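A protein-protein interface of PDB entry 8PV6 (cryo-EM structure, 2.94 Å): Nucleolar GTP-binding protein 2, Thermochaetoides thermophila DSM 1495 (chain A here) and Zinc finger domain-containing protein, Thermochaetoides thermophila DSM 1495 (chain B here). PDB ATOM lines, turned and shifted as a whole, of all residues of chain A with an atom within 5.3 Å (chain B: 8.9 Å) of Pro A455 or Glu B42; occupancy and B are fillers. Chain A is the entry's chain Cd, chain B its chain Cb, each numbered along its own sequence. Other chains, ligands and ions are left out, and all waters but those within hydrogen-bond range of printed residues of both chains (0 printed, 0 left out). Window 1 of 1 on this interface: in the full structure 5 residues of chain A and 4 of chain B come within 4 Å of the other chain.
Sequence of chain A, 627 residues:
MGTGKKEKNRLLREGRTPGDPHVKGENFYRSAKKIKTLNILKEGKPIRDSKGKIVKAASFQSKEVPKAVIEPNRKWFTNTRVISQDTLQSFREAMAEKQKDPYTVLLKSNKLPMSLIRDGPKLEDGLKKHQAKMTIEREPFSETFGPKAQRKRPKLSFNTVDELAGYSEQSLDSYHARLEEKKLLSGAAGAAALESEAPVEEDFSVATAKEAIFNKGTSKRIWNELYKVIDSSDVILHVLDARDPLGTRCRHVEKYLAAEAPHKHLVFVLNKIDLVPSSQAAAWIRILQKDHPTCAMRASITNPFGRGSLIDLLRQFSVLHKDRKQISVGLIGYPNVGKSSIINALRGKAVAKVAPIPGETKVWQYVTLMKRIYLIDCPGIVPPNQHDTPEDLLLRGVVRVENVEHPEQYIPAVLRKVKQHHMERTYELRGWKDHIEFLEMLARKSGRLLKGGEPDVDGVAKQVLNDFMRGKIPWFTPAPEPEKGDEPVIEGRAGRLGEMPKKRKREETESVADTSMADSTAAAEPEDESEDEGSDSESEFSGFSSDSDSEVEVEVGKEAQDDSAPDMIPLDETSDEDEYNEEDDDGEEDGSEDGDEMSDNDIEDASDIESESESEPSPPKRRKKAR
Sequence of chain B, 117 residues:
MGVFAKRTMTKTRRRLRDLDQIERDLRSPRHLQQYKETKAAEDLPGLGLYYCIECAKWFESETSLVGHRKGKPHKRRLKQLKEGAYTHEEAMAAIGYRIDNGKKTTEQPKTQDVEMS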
ATOM      1  N   GLU A 440       5.563 -13.905 -24.090  1.00  0.00           N
ATOM      2  CA  GLU A 440       6.943 -14.171 -23.696  1.00  0.00           C
ATOM      3  C   GLU A 440       7.895 -13.091 -24.198  1.00  0.00           C
ATOM      4  O   GLU A 440       8.737 -12.602 -23.436  1.00  0.00           O
ATOM      5  CB  GLU A 440       7.377 -15.546 -24.196  1.00  0.00           C
ATOM      6  CG  GLU A 440       6.792 -16.699 -23.405  1.00  0.00           C
ATOM      7  CD  GLU A 440       7.000 -18.030 -24.091  1.00  0.00           C
ATOM      8  OE1 GLU A 440       7.289 -18.032 -25.307  1.00  0.00           O
ATOM      9  OE2 GLU A 440       6.866 -19.074 -23.421  1.00  0.00           O
ATOM     10  N   ALA A 443       7.326  -9.943 -22.252  1.00  0.00           N
ATOM     11  CA  ALA A 443       7.934 -10.029 -20.929  1.00  0.00           C
ATOM     12  C   ALA A 443       9.441  -9.827 -21.000  1.00  0.00           C
ATOM     13  O   ALA A 443      10.024  -9.142 -20.154  1.00  0.00           O
ATOM     14  CB  ALA A 443       7.603 -11.378 -20.292  1.00  0.00           C
ATOM     15  N   ARG A 444      10.089 -10.417 -22.008  1.00  0.00           N
ATOM     16  CA  ARG A 444      11.532 -10.240 -22.148  1.00  0.00           C
ATOM     17  C   ARG A 444      11.887  -8.808 -22.530  1.00  0.00           C
ATOM     18  O   ARG A 444      12.951  -8.308 -22.147  1.00  0.00           O
ATOM     19  CB  ARG A 444      12.096 -11.222 -23.174  1.00  0.00           C
ATOM     20  CG  ARG A 444      11.904 -12.677 -22.805  1.00  0.00           C
ATOM     21  CD  ARG A 444      12.684 -13.588 -23.734  1.00  0.00           C
ATOM     22  NE  ARG A 444      12.141 -14.940 -23.743  1.00  0.00           N
ATOM     23  CZ  ARG A 444      11.301 -15.401 -24.659  1.00  0.00           C
ATOM     24  NH1 ARG A 444      10.903 -14.649 -25.671  1.00  0.00           N
ATOM     25  NH2 ARG A 444      10.853 -16.649 -24.559  1.00  0.00           N
ATOM     26  N   ARG A 448       9.686  -8.108 -17.380  1.00  0.00           N
ATOM     27  CA  ARG A 448       8.795  -8.828 -16.471  1.00  0.00           C
ATOM     28  C   ARG A 448       9.283 -10.270 -16.340  1.00  0.00           C
ATOM     29  O   ARG A 448       8.772 -11.205 -16.959  1.00  0.00           O
ATOM     30  CB  ARG A 448       7.357  -8.762 -16.966  1.00  0.00           C
ATOM     31  CG  ARG A 448       6.756  -7.361 -17.007  1.00  0.00           C
ATOM     32  CD  ARG A 448       6.136  -6.942 -15.675  1.00  0.00           C
ATOM     33  NE  ARG A 448       7.133  -6.648 -14.651  1.00  0.00           N
ATOM     34  CZ  ARG A 448       7.817  -5.515 -14.570  1.00  0.00           C
ATOM     35  NH1 ARG A 448       7.614  -4.523 -15.420  1.00  0.00           N
ATOM     36  NH2 ARG A 448       8.726  -5.377 -13.611  1.00  0.00           N
ATOM     37  N   LEU A 449      10.304 -10.436 -15.508  1.00  0.00           N
ATOM     38  CA  LEU A 449      10.971 -11.712 -15.320  1.00  0.00           C
ATOM     39  C   LEU A 449      10.814 -12.182 -13.882  1.00  0.00           C
ATOM     40  O   LEU A 449      10.798 -11.380 -12.945  1.00  0.00           O
ATOM     41  CB  LEU A 449      12.457 -11.608 -15.669  1.00  0.00           C
ATOM     42  CG  LEU A 449      12.779 -11.065 -17.061  1.00  0.00           C
ATOM     43  CD1 LEU A 449      14.267 -10.824 -17.213  1.00  0.00           C
ATOM     44  CD2 LEU A 449      12.278 -12.020 -18.128  1.00  0.00           C
ATOM     45  N   LEU A 450      10.692 -13.493 -13.719  1.00  0.00           N
ATOM     46  CA  LEU A 450      10.655 -14.117 -12.407  1.00  0.00           C
ATOM     47  C   LEU A 450      12.064 -14.521 -11.987  1.00  0.00           C
ATOM     48  O   LEU A 450      13.045 -14.270 -12.691  1.00  0.00           O
ATOM     49  CB  LEU A 450       9.723 -15.331 -12.415  1.00  0.00           C
ATOM     50  CG  LEU A 450       8.290 -15.070 -12.876  1.00  0.00           C
ATOM     51  CD1 LEU A 450       7.503 -16.365 -12.930  1.00  0.00           C
ATOM     52  CD2 LEU A 450       7.607 -14.062 -11.969  1.00  0.00           C
ATOM     53  N   GLY A 453      15.158 -15.940 -14.483  1.00  0.00           N
ATOM     54  CA  GLY A 453      15.017 -15.517 -15.867  1.00  0.00           C
ATOM     55  C   GLY A 453      13.781 -16.039 -16.562  1.00  0.00           C
ATOM     56  O   GLY A 453      13.731 -16.056 -17.796  1.00  0.00           O
ATOM     57  N   GLU A 454      12.780 -16.465 -15.806  1.00  0.00           N
ATOM     58  CA  GLU A 454      11.544 -16.978 -16.384  1.00  0.00           C
ATOM     59  C   GLU A 454      10.571 -15.830 -16.625  1.00  0.00           C
ATOM     60  O   GLU A 454      10.343 -15.025 -15.715  1.00  0.00           O
ATOM     61  CB  GLU A 454      10.910 -18.015 -15.471  1.00  0.00           C
ATOM     62  CG  GLU A 454       9.548 -18.503 -15.929  1.00  0.00           C
ATOM     63  CD  GLU A 454       8.967 -19.553 -15.007  1.00  0.00           C
ATOM     64  OE1 GLU A 454       9.696 -20.027 -14.111  1.00  0.00           O
ATOM     65  OE2 GLU A 454       7.781 -19.907 -15.179  1.00  0.00           O
ATOM     66  N   PRO A 455      10.013 -15.710 -17.830  1.00  0.00           N
ATOM     67  CA  PRO A 455       9.103 -14.593 -18.125  1.00  0.00           C
ATOM     68  C   PRO A 455       7.820 -14.662 -17.307  1.00  0.00           C
ATOM     69  O   PRO A 455       7.326 -15.743 -16.981  1.00  0.00           O
ATOM     70  CB  PRO A 455       8.826 -14.755 -19.625  1.00  0.00           C
ATOM     71  CG  PRO A 455       9.148 -16.176 -19.927  1.00  0.00           C
ATOM     72  CD  PRO A 455      10.276 -16.535 -19.019  1.00  0.00           C
ATOM     73  N   ASP A 456       7.282 -13.485 -16.976  1.00  0.00           N
ATOM     74  CA  ASP A 456       6.056 -13.372 -16.183  1.00  0.00           C
ATOM     75  C   ASP A 456       4.879 -13.202 -17.139  1.00  0.00           C
ATOM     76  O   ASP A 456       4.352 -12.104 -17.351  1.00  0.00           O
ATOM     77  CB  ASP A 456       6.160 -12.215 -15.198  1.00  0.00           C
ATOM     78  CG  ASP A 456       4.963 -12.127 -14.272  1.00  0.00           C
ATOM     79  OD1 ASP A 456       4.282 -13.154 -14.073  1.00  0.00           O
ATOM     80  OD2 ASP A 456       4.701 -11.028 -13.744  1.00  0.00           O
ATOM     81  N   VAL A 457       4.459 -14.331 -17.718  1.00  0.00           N
ATOM     82  CA  VAL A 457       3.384 -14.311 -18.706  1.00  0.00           C
ATOM     83  C   VAL A 457       2.060 -13.923 -18.058  1.00  0.00           C
ATOM     84  O   VAL A 457       1.224 -13.265 -18.685  1.00  0.00           O
ATOM     85  CB  VAL A 457       3.298 -15.664 -19.439  1.00  0.00           C
ATOM     86  CG1 VAL A 457       4.542 -15.884 -20.278  1.00  0.00           C
ATOM     87  CG2 VAL A 457       3.134 -16.812 -18.456  1.00  0.00           C
ATOM     88  N   LYS B  36      17.683 -32.373 -20.117  1.00  0.00           N
ATOM     89  CA  LYS B  36      17.130 -31.186 -20.759  1.00  0.00           C
ATOM     90  C   LYS B  36      15.663 -31.336 -21.172  1.00  0.00           C
ATOM     91  O   LYS B  36      14.953 -30.326 -21.198  1.00  0.00           O
ATOM     92  CB  LYS B  36      17.995 -30.783 -21.952  1.00  0.00           C
ATOM     93  CG  LYS B  36      19.337 -30.198 -21.527  1.00  0.00           C
ATOM     94  CD  LYS B  36      20.115 -29.616 -22.691  1.00  0.00           C
ATOM     95  CE  LYS B  36      21.341 -28.875 -22.189  1.00  0.00           C
ATOM     96  NZ  LYS B  36      22.147 -28.302 -23.299  1.00  0.00           N
ATOM     97  N   LYS B  39      13.250 -30.278 -18.406  1.00  0.00           N
ATOM     98  CA  LYS B  39      13.079 -28.851 -18.172  1.00  0.00           C
ATOM     99  C   LYS B  39      12.354 -28.221 -19.352  1.00  0.00           C
ATOM    100  O   LYS B  39      12.445 -28.712 -20.482  1.00  0.00           O
ATOM    101  CB  LYS B  39      14.430 -28.158 -17.965  1.00  0.00           C
ATOM    102  CG  LYS B  39      15.210 -28.661 -16.764  1.00  0.00           C
ATOM    103  CD  LYS B  39      14.533 -28.271 -15.465  1.00  0.00           C
ATOM    104  CE  LYS B  39      15.314 -28.785 -14.268  1.00  0.00           C
ATOM    105  NZ  LYS B  39      16.627 -28.100 -14.121  1.00  0.00           N
ATOM    106  N   ALA B  40      11.633 -27.134 -19.088  1.00  0.00           N
ATOM    107  CA  ALA B  40      10.938 -26.392 -20.136  1.00  0.00           C
ATOM    108  C   ALA B  40      11.890 -25.347 -20.705  1.00  0.00           C
ATOM    109  O   ALA B  40      12.444 -24.534 -19.959  1.00  0.00           O
ATOM    110  CB  ALA B  40       9.671 -25.746 -19.588  1.00  0.00           C
ATOM    111  N   ALA B  41      12.074 -25.365 -22.028  1.00  0.00           N
ATOM    112  CA  ALA B  41      13.093 -24.527 -22.655  1.00  0.00           C
ATOM    113  C   ALA B  41      12.732 -23.047 -22.601  1.00  0.00           C
ATOM    114  O   ALA B  41      13.617 -22.189 -22.503  1.00  0.00           O
ATOM    115  CB  ALA B  41      13.312 -24.966 -24.102  1.00  0.00           C
ATOM    116  N   GLU B  42      11.439 -22.726 -22.670  1.00  0.00           N
ATOM    117  CA  GLU B  42      11.019 -21.329 -22.662  1.00  0.00           C
ATOM    118  C   GLU B  42      11.168 -20.687 -21.289  1.00  0.00           C
ATOM    119  O   GLU B  42      11.190 -19.455 -21.194  1.00  0.00           O
ATOM    120  CB  GLU B  42       9.563 -21.174 -23.137  1.00  0.00           C
ATOM    121  CG  GLU B  42       9.179 -21.741 -24.526  1.00  0.00           C
ATOM    122  CD  GLU B  42       9.201 -23.262 -24.649  1.00  0.00           C
ATOM    123  OE1 GLU B  42       9.429 -23.958 -23.637  1.00  0.00           O
ATOM    124  OE2 GLU B  42       8.988 -23.762 -25.773  1.00  0.00           O
ATOM    125  N   ASP B  43      11.274 -21.485 -20.229  1.00  0.00           N
ATOM    126  CA  ASP B  43      11.373 -20.974 -18.871  1.00  0.00           C
ATOM    127  C   ASP B  43      12.809 -20.873 -18.374  1.00  0.00           C
ATOM    128  O   ASP B  43      13.022 -20.576 -17.195  1.00  0.00           O
ATOM    129  CB  ASP B  43      10.560 -21.856 -17.920  1.00  0.00           C
ATOM    130  CG  ASP B  43       9.068 -21.740 -18.154  1.00  0.00           C
ATOM    131  OD1 ASP B  43       8.620 -20.662 -18.599  1.00  0.00           O
ATOM    132  OD2 ASP B  43       8.346 -22.724 -17.893  1.00  0.00           O
ATOM    133  N   LEU B  44      13.790 -21.119 -19.233  1.00  0.00           N
ATOM    134  CA  LEU B  44      15.212 -21.087 -18.930  1.00  0.00           C
ATOM    135  C   LEU B  44      15.818 -19.752 -19.344  1.00  0.00           C
ATOM    136  O   LEU B  44      15.315 -19.109 -20.274  1.00  0.00           O
ATOM    137  CB  LEU B  44      15.932 -22.223 -19.656  1.00  0.00           C
ATOM    138  CG  LEU B  44      15.524 -23.628 -19.215  1.00  0.00           C
ATOM    139  CD1 LEU B  44      16.183 -24.676 -20.088  1.00  0.00           C
ATOM    140  CD2 LEU B  44      15.868 -23.849 -17.754  1.00  0.00           C
ATOM    141  N   PRO B  45      16.871 -19.292 -18.667  1.00  0.00           N
ATOM    142  CA  PRO B  45      17.534 -18.052 -19.092  1.00  0.00           C
ATOM    143  C   PRO B  45      18.193 -18.219 -20.453  1.00  0.00           C
ATOM    144  O   PRO B  45      18.842 -19.230 -20.728  1.00  0.00           O
ATOM    145  CB  PRO B  45      18.573 -17.805 -17.992  1.00  0.00           C
ATOM    146  CG  PRO B  45      18.135 -18.625 -16.840  1.00  0.00           C
ATOM    147  CD  PRO B  45      17.416 -19.805 -17.398  1.00  0.00           C
ATOM    148  N   GLY B  46      18.026 -17.210 -21.304  1.00  0.00           N
ATOM    149  CA  GLY B  46      18.580 -17.263 -22.643  1.00  0.00           C
ATOM    150  C   GLY B  46      17.952 -18.311 -23.532  1.00  0.00           C
ATOM    151  O   GLY B  46      18.603 -18.782 -24.471  1.00  0.00           O
ATOM    152  N   LEU B  47      16.706 -18.703 -23.236  1.00  0.00           N
ATOM    153  CA  LEU B  47      15.957 -19.730 -23.973  1.00  0.00           C
ATOM    154  C   LEU B  47      16.679 -21.076 -23.959  1.00  0.00           C
ATOM    155  O   LEU B  47      16.539 -21.890 -24.872  1.00  0.00           O
ATOM    156  CB  LEU B  47      15.648 -19.292 -25.411  1.00  0.00           C
ATOM    157  CG  LEU B  47      14.440 -18.393 -25.711  1.00  0.00           C
ATOM    158  CD1 LEU B  47      13.144 -19.111 -25.361  1.00  0.00           C
ATOM    159  CD2 LEU B  47      14.515 -17.028 -25.035  1.00  0.00           C
ATOM    160  N   GLY B  48      17.455 -21.315 -22.903  1.00  0.00           N
ATOM    161  CA  GLY B  48      18.187 -22.563 -22.774  1.00  0.00           C
ATOM    162  C   GLY B  48      19.318 -22.729 -23.764  1.00  0.00           C
ATOM    163  O   GLY B  48      19.779 -23.854 -23.983  1.00  0.00           O
ATOM    164  N   LEU B  49      19.784 -21.637 -24.367  1.00  0.00           N
ATOM    165  CA  LEU B  49      20.840 -21.710 -25.366  1.00  0.00           C
ATOM    166  C   LEU B  49      22.233 -21.597 -24.770  1.00  0.00           C
ATOM    167  O   LEU B  49      23.214 -21.887 -25.464  1.00  0.00           O
ATOM    168  CB  LEU B  49      20.653 -20.611 -26.415  1.00  0.00           C
ATOM    169  CG  LEU B  49      19.421 -20.726 -27.311  1.00  0.00           C
ATOM    170  CD1 LEU B  49      19.274 -19.489 -28.181  1.00  0.00           C
ATOM    171  CD2 LEU B  49      19.499 -21.979 -28.164  1.00  0.00           C
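The guanidinium group (NH2) of Arg A444 lies within salt-bridge range of the side-chain carboxylate (OE1) of Glu A440.
Glu A440 touches Glu B42 (OE2 to CB, 3.4 Å). Arg A444 touches Leu B47. CG of Glu A454 touches OD1 of Asp B43, 3.6 Å away. Pro A455 touches Glu B42.
Of chain B, only Glu B42 (3.8 Å) comes within 4 Å of Pro A455. Glu B42 touches two residues of chain A. Of the printed residues of chain A, Asp B43 touches Glu A454. Printed residues of chain A within 4 Å of Leu B47: Arg A444 (3.4 Å). Printed residues of chain B within 4 Å of Glu A440: Glu B42. Of the printed residues of chain B, Glu A454 touches Asp B43 (3.6 Å). Printed residues of chain B within 4 Å of Arg A444: Leu B47 (3.4 Å). The nearest residue of chain A that does not touch Glu B42 is Arg A444 (4.4 Å). The nearest printed residue of chain A that does not touch Asp B43 is Pro A455 (4.5 Å).
Of the 11 printed residues of chain A, 4 touch a printed residue of chain B. Printed residues of chain A that touch a printed residue of chain B: Glu A440, Arg A444, Glu A454 and Pro A455. Hydrophobic or aromatic side chains of chain A that line the printed part of chain B: Pro A455. Of the 12 printed residues of chain B, 3 touch a printed residue of chain A. Printed residues of chain B that touch a printed residue of chain A: Glu B42, Asp B43 and Leu B47.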
